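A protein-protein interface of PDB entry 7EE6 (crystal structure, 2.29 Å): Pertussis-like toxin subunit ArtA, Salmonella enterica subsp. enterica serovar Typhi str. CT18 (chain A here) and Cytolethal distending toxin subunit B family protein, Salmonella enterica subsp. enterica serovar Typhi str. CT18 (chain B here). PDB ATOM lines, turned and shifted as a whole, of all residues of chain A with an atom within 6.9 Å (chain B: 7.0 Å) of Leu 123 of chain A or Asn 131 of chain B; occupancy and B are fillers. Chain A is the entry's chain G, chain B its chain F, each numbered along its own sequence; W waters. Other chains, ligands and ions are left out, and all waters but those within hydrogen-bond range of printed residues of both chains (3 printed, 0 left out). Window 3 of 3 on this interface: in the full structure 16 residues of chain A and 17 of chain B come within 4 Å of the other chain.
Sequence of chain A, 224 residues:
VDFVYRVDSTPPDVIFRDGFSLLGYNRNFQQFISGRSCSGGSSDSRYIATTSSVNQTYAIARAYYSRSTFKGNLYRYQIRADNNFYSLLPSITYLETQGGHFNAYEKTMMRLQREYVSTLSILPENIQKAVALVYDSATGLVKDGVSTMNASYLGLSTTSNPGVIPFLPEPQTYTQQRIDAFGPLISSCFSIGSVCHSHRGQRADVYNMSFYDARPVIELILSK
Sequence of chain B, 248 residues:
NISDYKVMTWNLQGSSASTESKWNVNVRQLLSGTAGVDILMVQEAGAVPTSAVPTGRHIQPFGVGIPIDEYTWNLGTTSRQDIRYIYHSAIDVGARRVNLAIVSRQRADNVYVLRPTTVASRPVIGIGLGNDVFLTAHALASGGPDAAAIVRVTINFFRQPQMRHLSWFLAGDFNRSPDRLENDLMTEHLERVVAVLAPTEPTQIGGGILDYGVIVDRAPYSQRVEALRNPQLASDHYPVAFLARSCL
Water W1 lies within hydrogen-bond range of OG of Ser 121 of chain A and ND2 of Asn 1 of chain B.
Water W3 lies within hydrogen-bond range of the backbone carbonyl oxygen (O) of Asp 18 of chain A (2.8 Å), the backbone carbonyl oxygen (O) of Ile 122 of chain A (2.9 Å) and the side-chain amide nitrogen (ND2) of Asn 1 of chain B (2.9 Å).
Water W2 bridges N of Asn 1 of chain B (2.9 Å) and O of Ser 121 of chain A (3.1 Å).
Of the printed residues of chain B, Leu 123 of chain A touches Asn 1 (3.4 Å) and Asn 131 (3.1 Å).
Asn 131 of chain B touches one residue of chain A.
Of the printed residues of chain B, Glu 125 of chain A touches His 165.
Of the printed residues of chain A, His 165 of chain B touches Glu 125 (2.8 Å).
Printed residues of chain A within 4 Å of Asn 1 of chain B: Ser 121 (3.4 Å) and Leu 123 (3.4 Å).
Gly 128 of chain B touches none of the printed residues of chain A.
Ile 122 of chain A touches none of the printed residues of chain B.
The nearest printed residue of chain B that does not touch Leu 123 of chain A is Pro 220 of chain B (4.02 Å).
Among the printed residues, merely in contact across the chains: Asp 18 of chain A with Pro 220 of chain B (3.5 Å), Leu 120 of chain A with Tyr 5 of chain B (3.9 Å), Ser 121 of chain A with Asn 1 of chain B (3.4 Å), Leu 123 of chain A with Asn 1 of chain B (3.4 Å) and Leu 123 of chain A with Asn 131 of chain B (3.1 Å).
The backbone carbonyl oxygen of Asn 131 of chain B lies within hydrogen-bond range of the backbone NH of Ser 167 of chain B.
ND2 of Asn 131 of chain B sits at hydrogen-bond distance from O of His 165 of chain B (2.8 Å).
The backbone carbonyl oxygen (O) of Pro 220 of chain B lies within hydrogen-bond range of the side-chain amide nitrogen (ND2) of Asn 1 of chain B (3.4 Å).
The backbone carbonyl oxygen of Glu 125 of chain A lies within hydrogen-bond range of the guanidinium group of Arg 80 of chain A.
N of Asn 1 of chain B is in hydrogen-bond range of OD2 of Asp 132 of chain B (2.8 Å).
OE1 of Glu 125 of chain A lies within hydrogen-bond range of ND1 of His 165 of chain B, at 2.8 Å.
Of the 18 printed residues of chain B, 5 touch a printed residue of chain A.
Hydrophobic or aromatic side chains of chain B that line the printed part of chain A: Tyr 5, His 165 and Pro 220.
Printed residues of chain A that touch a printed residue of chain B: Asp 18, Leu 120, Ser 121, Leu 123 and Glu 125.
Hydrophobic or aromatic side chains of chain A within 4 Å of the printed part of chain B: Leu 120 and Leu 123.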
ATOM      1  N   ILE A  15     -16.811   1.440  21.490  1.00  0.00           N
ATOM      2  CA  ILE A  15     -16.090   2.650  21.854  1.00  0.00           C
ATOM      3  C   ILE A  15     -14.682   2.317  22.336  1.00  0.00           C
ATOM      4  O   ILE A  15     -13.726   3.034  22.026  1.00  0.00           O
ATOM      5  CB  ILE A  15     -16.879   3.456  22.905  1.00  0.00           C
ATOM      6  CG1 ILE A  15     -18.167   4.014  22.292  1.00  0.00           C
ATOM      7  CG2 ILE A  15     -15.999   4.568  23.503  1.00  0.00           C
ATOM      8  CD1 ILE A  15     -17.936   5.011  21.117  1.00  0.00           C
ATOM      9  N   PHE A  16     -14.530   1.239  23.112  1.00  0.00           N
ATOM     10  CA  PHE A  16     -13.205   0.832  23.586  1.00  0.00           C
ATOM     11  C   PHE A  16     -12.293   0.390  22.453  1.00  0.00           C
ATOM     12  O   PHE A  16     -11.077   0.306  22.655  1.00  0.00           O
ATOM     13  CB  PHE A  16     -13.305  -0.310  24.599  1.00  0.00           C
ATOM     14  CG  PHE A  16     -13.993   0.075  25.862  1.00  0.00           C
ATOM     15  CD1 PHE A  16     -14.187   1.420  26.176  1.00  0.00           C
ATOM     16  CD2 PHE A  16     -14.454  -0.895  26.742  1.00  0.00           C
ATOM     17  CE1 PHE A  16     -14.818   1.786  27.348  1.00  0.00           C
ATOM     18  CE2 PHE A  16     -15.096  -0.535  27.917  1.00  0.00           C
ATOM     19  CZ  PHE A  16     -15.275   0.804  28.220  1.00  0.00           C
ATOM     20  N   ASP A  18     -12.632   1.936  19.101  1.00  0.00           N
ATOM     21  CA  ASP A  18     -12.442   3.035  18.159  1.00  0.00           C
ATOM     22  C   ASP A  18     -12.163   4.382  18.805  1.00  0.00           C
ATOM     23  O   ASP A  18     -11.522   5.231  18.177  1.00  0.00           O
ATOM     24  CB  ASP A  18     -13.682   3.202  17.266  1.00  0.00           C
ATOM     25  CG  ASP A  18     -13.993   1.969  16.454  1.00  0.00           C
ATOM     26  OD1 ASP A  18     -13.048   1.309  15.974  1.00  0.00           O
ATOM     27  OD2 ASP A  18     -15.191   1.668  16.291  1.00  0.00           O
ATOM     28  N   GLY A  19     -12.649   4.608  20.021  1.00  0.00           N
ATOM     29  CA  GLY A  19     -12.632   5.942  20.582  1.00  0.00           C
ATOM     30  C   GLY A  19     -13.693   6.828  19.944  1.00  0.00           C
ATOM     31  O   GLY A  19     -14.644   6.362  19.297  1.00  0.00           O
ATOM     32  N   PHE A  20     -13.512   8.135  20.121  1.00  0.00           N
ATOM     33  CA  PHE A  20     -14.424   9.146  19.607  1.00  0.00           C
ATOM     34  C   PHE A  20     -13.726  10.000  18.553  1.00  0.00           C
ATOM     35  O   PHE A  20     -12.582  10.432  18.746  1.00  0.00           O
ATOM     36  CB  PHE A  20     -14.914  10.057  20.724  1.00  0.00           C
ATOM     37  CG  PHE A  20     -15.738   9.378  21.760  1.00  0.00           C
ATOM     38  CD1 PHE A  20     -16.999   8.885  21.451  1.00  0.00           C
ATOM     39  CD2 PHE A  20     -15.289   9.290  23.070  1.00  0.00           C
ATOM     40  CE1 PHE A  20     -17.795   8.287  22.423  1.00  0.00           C
ATOM     41  CE2 PHE A  20     -16.080   8.682  24.063  1.00  0.00           C
ATOM     42  CZ  PHE A  20     -17.335   8.180  23.734  1.00  0.00           C
ATOM     43  N   ILE A  79     -13.311   9.531  30.818  1.00  0.00           N
ATOM     44  CA  ILE A  79     -12.201   9.834  29.929  1.00  0.00           C
ATOM     45  C   ILE A  79     -11.115  10.556  30.715  1.00  0.00           C
ATOM     46  O   ILE A  79     -11.387  11.571  31.370  1.00  0.00           O
ATOM     47  CB  ILE A  79     -12.664  10.696  28.739  1.00  0.00           C
ATOM     48  CG1 ILE A  79     -13.816  10.022  27.984  1.00  0.00           C
ATOM     49  CG2 ILE A  79     -11.472  11.104  27.834  1.00  0.00           C
ATOM     50  CD1 ILE A  79     -14.625  11.024  27.150  1.00  0.00           C
ATOM     51  N   ARG A  80      -9.884  10.044  30.634  1.00  0.00           N
ATOM     52  CA  ARG A  80      -8.733  10.735  31.199  1.00  0.00           C
ATOM     53  C   ARG A  80      -8.363  11.913  30.299  1.00  0.00           C
ATOM     54  O   ARG A  80      -8.182  11.747  29.090  1.00  0.00           O
ATOM     55  CB  ARG A  80      -7.544   9.782  31.349  1.00  0.00           C
ATOM     56  CG  ARG A  80      -6.221  10.468  31.686  1.00  0.00           C
ATOM     57  CD  ARG A  80      -5.075   9.464  31.929  1.00  0.00           C
ATOM     58  NE  ARG A  80      -4.965   8.503  30.836  1.00  0.00           N
ATOM     59  CZ  ARG A  80      -4.388   8.756  29.662  1.00  0.00           C
ATOM     60  NH1 ARG A  80      -3.842   9.947  29.422  1.00  0.00           N
ATOM     61  NH2 ARG A  80      -4.362   7.807  28.726  1.00  0.00           N
ATOM     62  N   PHE A  85      -6.885  18.524  25.972  1.00  0.00           N
ATOM     63  CA  PHE A  85      -8.183  18.912  26.512  1.00  0.00           C
ATOM     64  C   PHE A  85      -8.060  20.313  27.098  1.00  0.00           C
ATOM     65  O   PHE A  85      -7.211  20.541  27.961  1.00  0.00           O
ATOM     66  CB  PHE A  85      -8.647  17.932  27.587  1.00  0.00           C
ATOM     67  CG  PHE A  85      -9.005  16.557  27.064  1.00  0.00           C
ATOM     68  CD1 PHE A  85      -8.039  15.730  26.495  1.00  0.00           C
ATOM     69  CD2 PHE A  85     -10.296  16.072  27.186  1.00  0.00           C
ATOM     70  CE1 PHE A  85      -8.370  14.463  26.040  1.00  0.00           C
ATOM     71  CE2 PHE A  85     -10.622  14.799  26.735  1.00  0.00           C
ATOM     72  CZ  PHE A  85      -9.651  13.998  26.165  1.00  0.00           C
ATOM     73  N   LEU A 120      -8.286  16.920  19.468  1.00  0.00           N
ATOM     74  CA  LEU A 120      -8.029  15.709  18.696  1.00  0.00           C
ATOM     75  C   LEU A 120      -9.105  14.674  19.000  1.00  0.00           C
ATOM     76  O   LEU A 120      -9.843  14.775  19.997  1.00  0.00           O
ATOM     77  CB  LEU A 120      -6.648  15.118  19.023  1.00  0.00           C
ATOM     78  CG  LEU A 120      -5.415  15.925  18.613  1.00  0.00           C
ATOM     79  CD1 LEU A 120      -4.153  15.202  19.072  1.00  0.00           C
ATOM     80  CD2 LEU A 120      -5.398  16.112  17.099  1.00  0.00           C
ATOM     81  N   SER A 121      -9.174  13.655  18.144  1.00  0.00           N
ATOM     82  CA  SER A 121      -9.978  12.485  18.472  1.00  0.00           C
ATOM     83  C   SER A 121      -9.535  11.920  19.821  1.00  0.00           C
ATOM     84  O   SER A 121      -8.383  12.072  20.238  1.00  0.00           O
ATOM     85  CB  SER A 121      -9.830  11.413  17.398  1.00  0.00           C
ATOM     86  OG  SER A 121     -10.471  11.804  16.198  1.00  0.00           O
ATOM     87  N   ILE A 122     -10.454  11.250  20.502  1.00  0.00           N
ATOM     88  CA  ILE A 122     -10.179  10.675  21.808  1.00  0.00           C
ATOM     89  C   ILE A 122      -9.937   9.191  21.604  1.00  0.00           C
ATOM     90  O   ILE A 122     -10.829   8.473  21.132  1.00  0.00           O
ATOM     91  CB  ILE A 122     -11.335  10.921  22.791  1.00  0.00           C
ATOM     92  CG1 ILE A 122     -11.568  12.427  23.023  1.00  0.00           C
ATOM     93  CG2 ILE A 122     -11.104  10.154  24.109  1.00  0.00           C
ATOM     94  CD1 ILE A 122     -12.730  12.721  24.002  1.00  0.00           C
ATOM     95  N   LEU A 123      -8.725   8.732  21.954  1.00  0.00           N
ATOM     96  CA  LEU A 123      -8.293   7.350  21.762  1.00  0.00           C
ATOM     97  C   LEU A 123      -8.865   6.432  22.845  1.00  0.00           C
ATOM     98  O   LEU A 123      -9.124   6.868  23.975  1.00  0.00           O
ATOM     99  CB  LEU A 123      -6.770   7.263  21.787  1.00  0.00           C
ATOM    100  CG  LEU A 123      -6.019   7.692  20.518  1.00  0.00           C
ATOM    101  CD1 LEU A 123      -4.540   7.779  20.823  1.00  0.00           C
ATOM    102  CD2 LEU A 123      -6.270   6.716  19.352  1.00  0.00           C
ATOM    103  N   PRO A 124      -9.062   5.155  22.525  1.00  0.00           N
ATOM    104  CA  PRO A 124      -9.426   4.189  23.572  1.00  0.00           C
ATOM    105  C   PRO A 124      -8.466   4.188  24.751  1.00  0.00           C
ATOM    106  O   PRO A 124      -8.877   3.879  25.880  1.00  0.00           O
ATOM    107  CB  PRO A 124      -9.402   2.844  22.828  1.00  0.00           C
ATOM    108  CG  PRO A 124      -9.626   3.210  21.365  1.00  0.00           C
ATOM    109  CD  PRO A 124      -8.963   4.540  21.187  1.00  0.00           C
ATOM    110  N   GLU A 125      -7.198   4.530  24.522  1.00  0.00           N
ATOM    111  CA  GLU A 125      -6.221   4.599  25.601  1.00  0.00           C
ATOM    112  C   GLU A 125      -6.625   5.593  26.688  1.00  0.00           C
ATOM    113  O   GLU A 125      -6.215   5.432  27.845  1.00  0.00           O
ATOM    114  CB  GLU A 125      -4.846   4.965  25.020  1.00  0.00           C
ATOM    115  CG  GLU A 125      -4.132   3.807  24.285  1.00  0.00           C
ATOM    116  CD  GLU A 125      -4.576   3.607  22.822  1.00  0.00           C
ATOM    117  OE1 GLU A 125      -3.884   2.866  22.088  1.00  0.00           O
ATOM    118  OE2 GLU A 125      -5.605   4.170  22.396  1.00  0.00           O
ATOM    119  N   ASN A 126      -7.415   6.610  26.352  1.00  0.00           N
ATOM    120  CA  ASN A 126      -7.868   7.595  27.335  1.00  0.00           C
ATOM    121  C   ASN A 126      -9.171   7.204  28.033  1.00  0.00           C
ATOM    122  O   ASN A 126      -9.536   7.844  29.030  1.00  0.00           O
ATOM    123  CB  ASN A 126      -8.059   8.962  26.664  1.00  0.00           C
ATOM    124  CG  ASN A 126      -6.749   9.625  26.286  1.00  0.00           C
ATOM    125  OD1 ASN A 126      -6.055   9.170  25.386  1.00  0.00           O
ATOM    126  ND2 ASN A 126      -6.420  10.728  26.953  1.00  0.00           N
ATOM    127  N   ILE A 127      -9.879   6.187  27.544  1.00  0.00           N
ATOM    128  CA  ILE A 127     -11.222   5.872  28.023  1.00  0.00           C
ATOM    129  C   ILE A 127     -11.114   4.792  29.100  1.00  0.00           C
ATOM    130  O   ILE A 127     -10.807   3.633  28.816  1.00  0.00           O
ATOM    131  CB  ILE A 127     -12.139   5.457  26.864  1.00  0.00           C
ATOM    132  CG1 ILE A 127     -12.185   6.593  25.820  1.00  0.00           C
ATOM    133  CG2 ILE A 127     -13.538   5.104  27.355  1.00  0.00           C
ATOM    134  CD1 ILE A 127     -12.942   6.272  24.539  1.00  0.00           C
ATOM    135  N   ASN A 150     -12.231  -0.672  30.719  1.00  0.00           N
ATOM    136  CA  ASN A 150     -11.565  -0.824  29.422  1.00  0.00           C
ATOM    137  C   ASN A 150     -10.151  -1.372  29.628  1.00  0.00           C
ATOM    138  O   ASN A 150      -9.275  -0.673  30.139  1.00  0.00           O
ATOM    139  CB  ASN A 150     -11.540   0.516  28.685  1.00  0.00           C
ATOM    140  CG  ASN A 150     -10.820   0.440  27.344  1.00  0.00           C
ATOM    141  OD1 ASN A 150     -10.664  -0.641  26.771  1.00  0.00           O
ATOM    142  ND2 ASN A 150     -10.400   1.601  26.825  1.00  0.00           N
ATOM    143  N   ASN B   1      -5.703  11.244  15.764  1.00  0.00           N
ATOM    144  CA  ASN B   1      -5.983  10.330  14.676  1.00  0.00           C
ATOM    145  C   ASN B   1      -5.618  11.000  13.357  1.00  0.00           C
ATOM    146  O   ASN B   1      -5.564  12.227  13.289  1.00  0.00           O
ATOM    147  CB  ASN B   1      -7.465   9.908  14.697  1.00  0.00           C
ATOM    148  CG  ASN B   1      -7.800   8.977  15.863  1.00  0.00           C
ATOM    149  OD1 ASN B   1      -6.965   8.712  16.734  1.00  0.00           O
ATOM    150  ND2 ASN B   1      -9.031   8.473  15.881  1.00  0.00           N
ATOM    151  N   ILE B   2      -5.377  10.200  12.306  1.00  0.00           N
ATOM    152  CA  ILE B   2      -5.001  10.777  11.015  1.00  0.00           C
ATOM    153  C   ILE B   2      -6.082  11.732  10.523  1.00  0.00           C
ATOM    154  O   ILE B   2      -5.792  12.808   9.984  1.00  0.00           O
ATOM    155  CB  ILE B   2      -4.734   9.665   9.985  1.00  0.00           C
ATOM    156  CG1 ILE B   2      -3.808   8.599  10.582  1.00  0.00           C
ATOM    157  CG2 ILE B   2      -4.179  10.263   8.682  1.00  0.00           C
ATOM    158  CD1 ILE B   2      -2.411   9.109  10.932  1.00  0.00           C
ATOM    159  N   TYR B   5      -6.150  15.678  11.005  1.00  0.00           N
ATOM    160  CA  TYR B   5      -5.237  16.583  10.313  1.00  0.00           C
ATOM    161  C   TYR B   5      -5.596  16.713   8.837  1.00  0.00           C
ATOM    162  O   TYR B   5      -6.091  15.769   8.210  1.00  0.00           O
ATOM    163  CB  TYR B   5      -3.789  16.096  10.401  1.00  0.00           C
ATOM    164  CG  TYR B   5      -3.252  16.035  11.794  1.00  0.00           C
ATOM    165  CD1 TYR B   5      -3.550  14.956  12.626  1.00  0.00           C
ATOM    166  CD2 TYR B   5      -2.428  17.049  12.284  1.00  0.00           C
ATOM    167  CE1 TYR B   5      -3.036  14.887  13.918  1.00  0.00           C
ATOM    168  CE2 TYR B   5      -1.919  16.996  13.573  1.00  0.00           C
ATOM    169  CZ  TYR B   5      -2.228  15.918  14.384  1.00  0.00           C
ATOM    170  OH  TYR B   5      -1.731  15.875  15.666  1.00  0.00           O
ATOM    171  N   ASP B 109       7.382  15.453  18.045  1.00  0.00           N
ATOM    172  CA  ASP B 109       7.867  14.768  19.239  1.00  0.00           C
ATOM    173  C   ASP B 109       8.988  13.810  18.896  1.00  0.00           C
ATOM    174  O   ASP B 109       9.992  13.736  19.610  1.00  0.00           O
ATOM    175  CB  ASP B 109       6.727  14.017  19.922  1.00  0.00           C
ATOM    176  CG  ASP B 109       5.553  14.908  20.231  1.00  0.00           C
ATOM    177  OD1 ASP B 109       5.784  16.049  20.682  1.00  0.00           O
ATOM    178  OD2 ASP B 109       4.399  14.473  20.017  1.00  0.00           O
ATOM    179  N   GLY B 128       6.534  12.121  14.295  1.00  0.00           N
ATOM    180  CA  GLY B 128       5.480  11.733  15.211  1.00  0.00           C
ATOM    181  C   GLY B 128       4.919  12.951  15.968  1.00  0.00           C
ATOM    182  O   GLY B 128       5.679  13.742  16.520  1.00  0.00           O
ATOM    183  N   LEU B 129       3.597  13.045  15.973  1.00  0.00           N
ATOM    184  CA  LEU B 129       2.879  14.026  16.782  1.00  0.00           C
ATOM    185  C   LEU B 129       1.942  13.232  17.681  1.00  0.00           C
ATOM    186  O   LEU B 129       0.910  12.729  17.222  1.00  0.00           O
ATOM    187  CB  LEU B 129       2.118  15.023  15.916  1.00  0.00           C
ATOM    188  CG  LEU B 129       2.983  15.895  14.999  1.00  0.00           C
ATOM    189  CD1 LEU B 129       2.146  16.660  13.985  1.00  0.00           C
ATOM    190  CD2 LEU B 129       3.820  16.858  15.835  1.00  0.00           C
ATOM    191  N   GLY B 130       2.302  13.097  18.950  1.00  0.00           N
ATOM    192  CA  GLY B 130       1.468  12.314  19.844  1.00  0.00           C
ATOM    193  C   GLY B 130       1.381  10.876  19.370  1.00  0.00           C
ATOM    194  O   GLY B 130       2.399  10.185  19.207  1.00  0.00           O
ATOM    195  N   ASN B 131       0.156  10.410  19.104  1.00  0.00           N
ATOM    196  CA  ASN B 131      -0.005   9.012  18.766  1.00  0.00           C
ATOM    197  C   ASN B 131      -0.003   8.824  17.233  1.00  0.00           C
ATOM    198  O   ASN B 131      -0.275   7.722  16.730  1.00  0.00           O
ATOM    199  CB  ASN B 131      -1.336   8.471  19.261  1.00  0.00           C
ATOM    200  CG  ASN B 131      -1.236   7.014  19.627  1.00  0.00           C
ATOM    201  OD1 ASN B 131      -0.112   6.553  19.884  1.00  0.00           O
ATOM    202  ND2 ASN B 131      -2.282   6.240  19.389  1.00  0.00           N
ATOM    203  N   ASP B 132       0.243   9.887  16.480  1.00  0.00           N
ATOM    204  CA  ASP B 132       0.142   9.889  15.025  1.00  0.00           C
ATOM    205  C   ASP B 132       1.516  10.107  14.415  1.00  0.00           C
ATOM    206  O   ASP B 132       2.264  10.992  14.860  1.00  0.00           O
ATOM    207  CB  ASP B 132      -0.837  10.971  14.553  1.00  0.00           C
ATOM    208  CG  ASP B 132      -2.250  10.704  15.037  1.00  0.00           C
ATOM    209  OD1 ASP B 132      -2.674   9.527  14.966  1.00  0.00           O
ATOM    210  OD2 ASP B 132      -2.933  11.652  15.511  1.00  0.00           O
ATOM    211  N   VAL B 133       1.834   9.304  13.398  1.00  0.00           N
ATOM    212  CA  VAL B 133       3.083   9.400  12.654  1.00  0.00           C
ATOM    213  C   VAL B 133       2.759   9.618  11.183  1.00  0.00           C
ATOM    214  O   VAL B 133       1.943   8.886  10.611  1.00  0.00           O
ATOM    215  CB  VAL B 133       3.946   8.142  12.835  1.00  0.00           C
ATOM    216  CG1 VAL B 133       5.253   8.261  12.056  1.00  0.00           C
ATOM    217  CG2 VAL B 133       4.206   7.881  14.314  1.00  0.00           C
ATOM    218  N   PHE B 134       3.422  10.601  10.568  1.00  0.00           N
ATOM    219  CA  PHE B 134       3.234  10.969   9.170  1.00  0.00           C
ATOM    220  C   PHE B 134       4.567  10.802   8.457  1.00  0.00           C
ATOM    221  O   PHE B 134       5.563  11.420   8.852  1.00  0.00           O
ATOM    222  CB  PHE B 134       2.732  12.409   9.050  1.00  0.00           C
ATOM    223  CG  PHE B 134       1.482  12.665   9.828  1.00  0.00           C
ATOM    224  CD1 PHE B 134       1.546  13.068  11.152  1.00  0.00           C
ATOM    225  CD2 PHE B 134       0.240  12.467   9.246  1.00  0.00           C
ATOM    226  CE1 PHE B 134       0.391  13.283  11.884  1.00  0.00           C
ATOM    227  CE2 PHE B 134      -0.923  12.678   9.970  1.00  0.00           C
ATOM    228  CZ  PHE B 134      -0.849  13.090  11.292  1.00  0.00           C
ATOM    229  N   MET B 163       5.638   0.042  19.211  1.00  0.00           N
ATOM    230  CA  MET B 163       5.200   0.995  18.212  1.00  0.00           C
ATOM    231  C   MET B 163       3.758   0.765  17.806  1.00  0.00           C
ATOM    232  O   MET B 163       3.210   1.561  17.035  1.00  0.00           O
ATOM    233  CB  MET B 163       6.102   0.913  16.976  1.00  0.00           C
ATOM    234  CG  MET B 163       7.563   1.187  17.274  1.00  0.00           C
ATOM    235  SD  MET B 163       7.827   2.960  17.365  1.00  0.00           S
ATOM    236  CE  MET B 163       9.520   3.017  17.908  1.00  0.00           C
ATOM    237  N   ARG B 164       3.133  -0.300  18.308  1.00  0.00           N
ATOM    238  CA  ARG B 164       1.825  -0.710  17.816  1.00  0.00           C
ATOM    239  C   ARG B 164       0.708   0.219  18.252  1.00  0.00           C
ATOM    240  O   ARG B 164      -0.371   0.167  17.663  1.00  0.00           O
ATOM    241  CB  ARG B 164       1.523  -2.145  18.259  1.00  0.00           C
ATOM    242  CG  ARG B 164       1.438  -2.223  19.763  1.00  0.00           C
ATOM    243  CD  ARG B 164       1.188  -3.613  20.305  1.00  0.00           C
ATOM    244  NE  ARG B 164       1.164  -3.551  21.770  1.00  0.00           N
ATOM    245  CZ  ARG B 164       0.917  -4.587  22.568  1.00  0.00           C
ATOM    246  NH1 ARG B 164       0.641  -5.778  22.046  1.00  0.00           N
ATOM    247  NH2 ARG B 164       0.915  -4.429  23.885  1.00  0.00           N
ATOM    248  N   HIS B 165       0.932   1.044  19.275  1.00  0.00           N
ATOM    249  CA  HIS B 165      -0.074   2.022  19.675  1.00  0.00           C
ATOM    250  C   HIS B 165      -0.256   3.123  18.636  1.00  0.00           C
ATOM    251  O   HIS B 165      -1.307   3.772  18.612  1.00  0.00           O
ATOM    252  CB  HIS B 165       0.295   2.687  21.013  1.00  0.00           C
ATOM    253  CG  HIS B 165      -0.090   1.905  22.236  1.00  0.00           C
ATOM    254  ND1 HIS B 165      -1.401   1.654  22.585  1.00  0.00           N
ATOM    255  CD2 HIS B 165       0.671   1.337  23.203  1.00  0.00           C
ATOM    256  CE1 HIS B 165      -1.430   0.957  23.707  1.00  0.00           C
ATOM    257  NE2 HIS B 165      -0.186   0.749  24.101  1.00  0.00           N
ATOM    258  N   LEU B 166       0.747   3.361  17.799  1.00  0.00           N
ATOM    259  CA  LEU B 166       0.744   4.503  16.900  1.00  0.00           C
ATOM    260  C   LEU B 166      -0.133   4.258  15.674  1.00  0.00           C
ATOM    261  O   LEU B 166      -0.162   3.153  15.120  1.00  0.00           O
ATOM    262  CB  LEU B 166       2.177   4.815  16.456  1.00  0.00           C
ATOM    263  CG  LEU B 166       3.160   5.187  17.564  1.00  0.00           C
ATOM    264  CD1 LEU B 166       4.618   5.112  17.090  1.00  0.00           C
ATOM    265  CD2 LEU B 166       2.825   6.588  18.043  1.00  0.00           C
ATOM    266  N   SER B 167      -0.869   5.296  15.265  1.00  0.00           N
ATOM    267  CA  SER B 167      -1.405   5.389  13.909  1.00  0.00           C
ATOM    268  C   SER B 167      -0.361   6.009  12.995  1.00  0.00           C
ATOM    269  O   SER B 167       0.208   7.063  13.315  1.00  0.00           O
ATOM    270  CB  SER B 167      -2.681   6.230  13.844  1.00  0.00           C
ATOM    271  OG  SER B 167      -3.652   5.791  14.762  1.00  0.00           O
ATOM    272  N   TRP B 168      -0.117   5.373  11.853  1.00  0.00           N
ATOM    273  CA  TRP B 168       0.783   5.968  10.880  1.00  0.00           C
ATOM    274  C   TRP B 168       0.113   6.089   9.523  1.00  0.00           C
ATOM    275  O   TRP B 168      -0.778   5.310   9.170  1.00  0.00           O
ATOM    276  CB  TRP B 168       2.099   5.199  10.761  1.00  0.00           C
ATOM    277  CG  TRP B 168       2.039   3.812  10.223  1.00  0.00           C
ATOM    278  CD1 TRP B 168       2.090   2.652  10.951  1.00  0.00           C
ATOM    279  CD2 TRP B 168       2.010   3.415   8.839  1.00  0.00           C
ATOM    280  NE1 TRP B 168       2.096   1.565  10.113  1.00  0.00           N
ATOM    281  CE2 TRP B 168       2.041   2.000   8.812  1.00  0.00           C
ATOM    282  CE3 TRP B 168       1.962   4.115   7.623  1.00  0.00           C
ATOM    283  CZ2 TRP B 168       1.980   1.268   7.616  1.00  0.00           C
ATOM    284  CZ3 TRP B 168       1.918   3.392   6.433  1.00  0.00           C
ATOM    285  CH2 TRP B 168       1.933   1.978   6.439  1.00  0.00           C
ATOM    286  N   PRO B 220      -7.401   4.104  14.187  1.00  0.00           N
ATOM    287  CA  PRO B 220      -8.827   4.382  14.399  1.00  0.00           C
ATOM    288  C   PRO B 220      -9.353   5.411  13.397  1.00  0.00           C
ATOM    289  O   PRO B 220      -8.713   6.433  13.126  1.00  0.00           O
ATOM    290  CB  PRO B 220      -8.873   4.889  15.845  1.00  0.00           C
ATOM    291  CG  PRO B 220      -7.652   4.259  16.490  1.00  0.00           C
ATOM    292  CD  PRO B 220      -6.608   4.242  15.424  1.00  0.00           C
HETATM  293  O   HOH W   1     -10.760  10.097  14.126  1.00  0.00           O
HETATM  294  O   HOH W   2      -5.993  11.060  18.628  1.00  0.00           O
HETATM  295  O   HOH W   3     -10.021   7.556  18.495  1.00  0.00           O
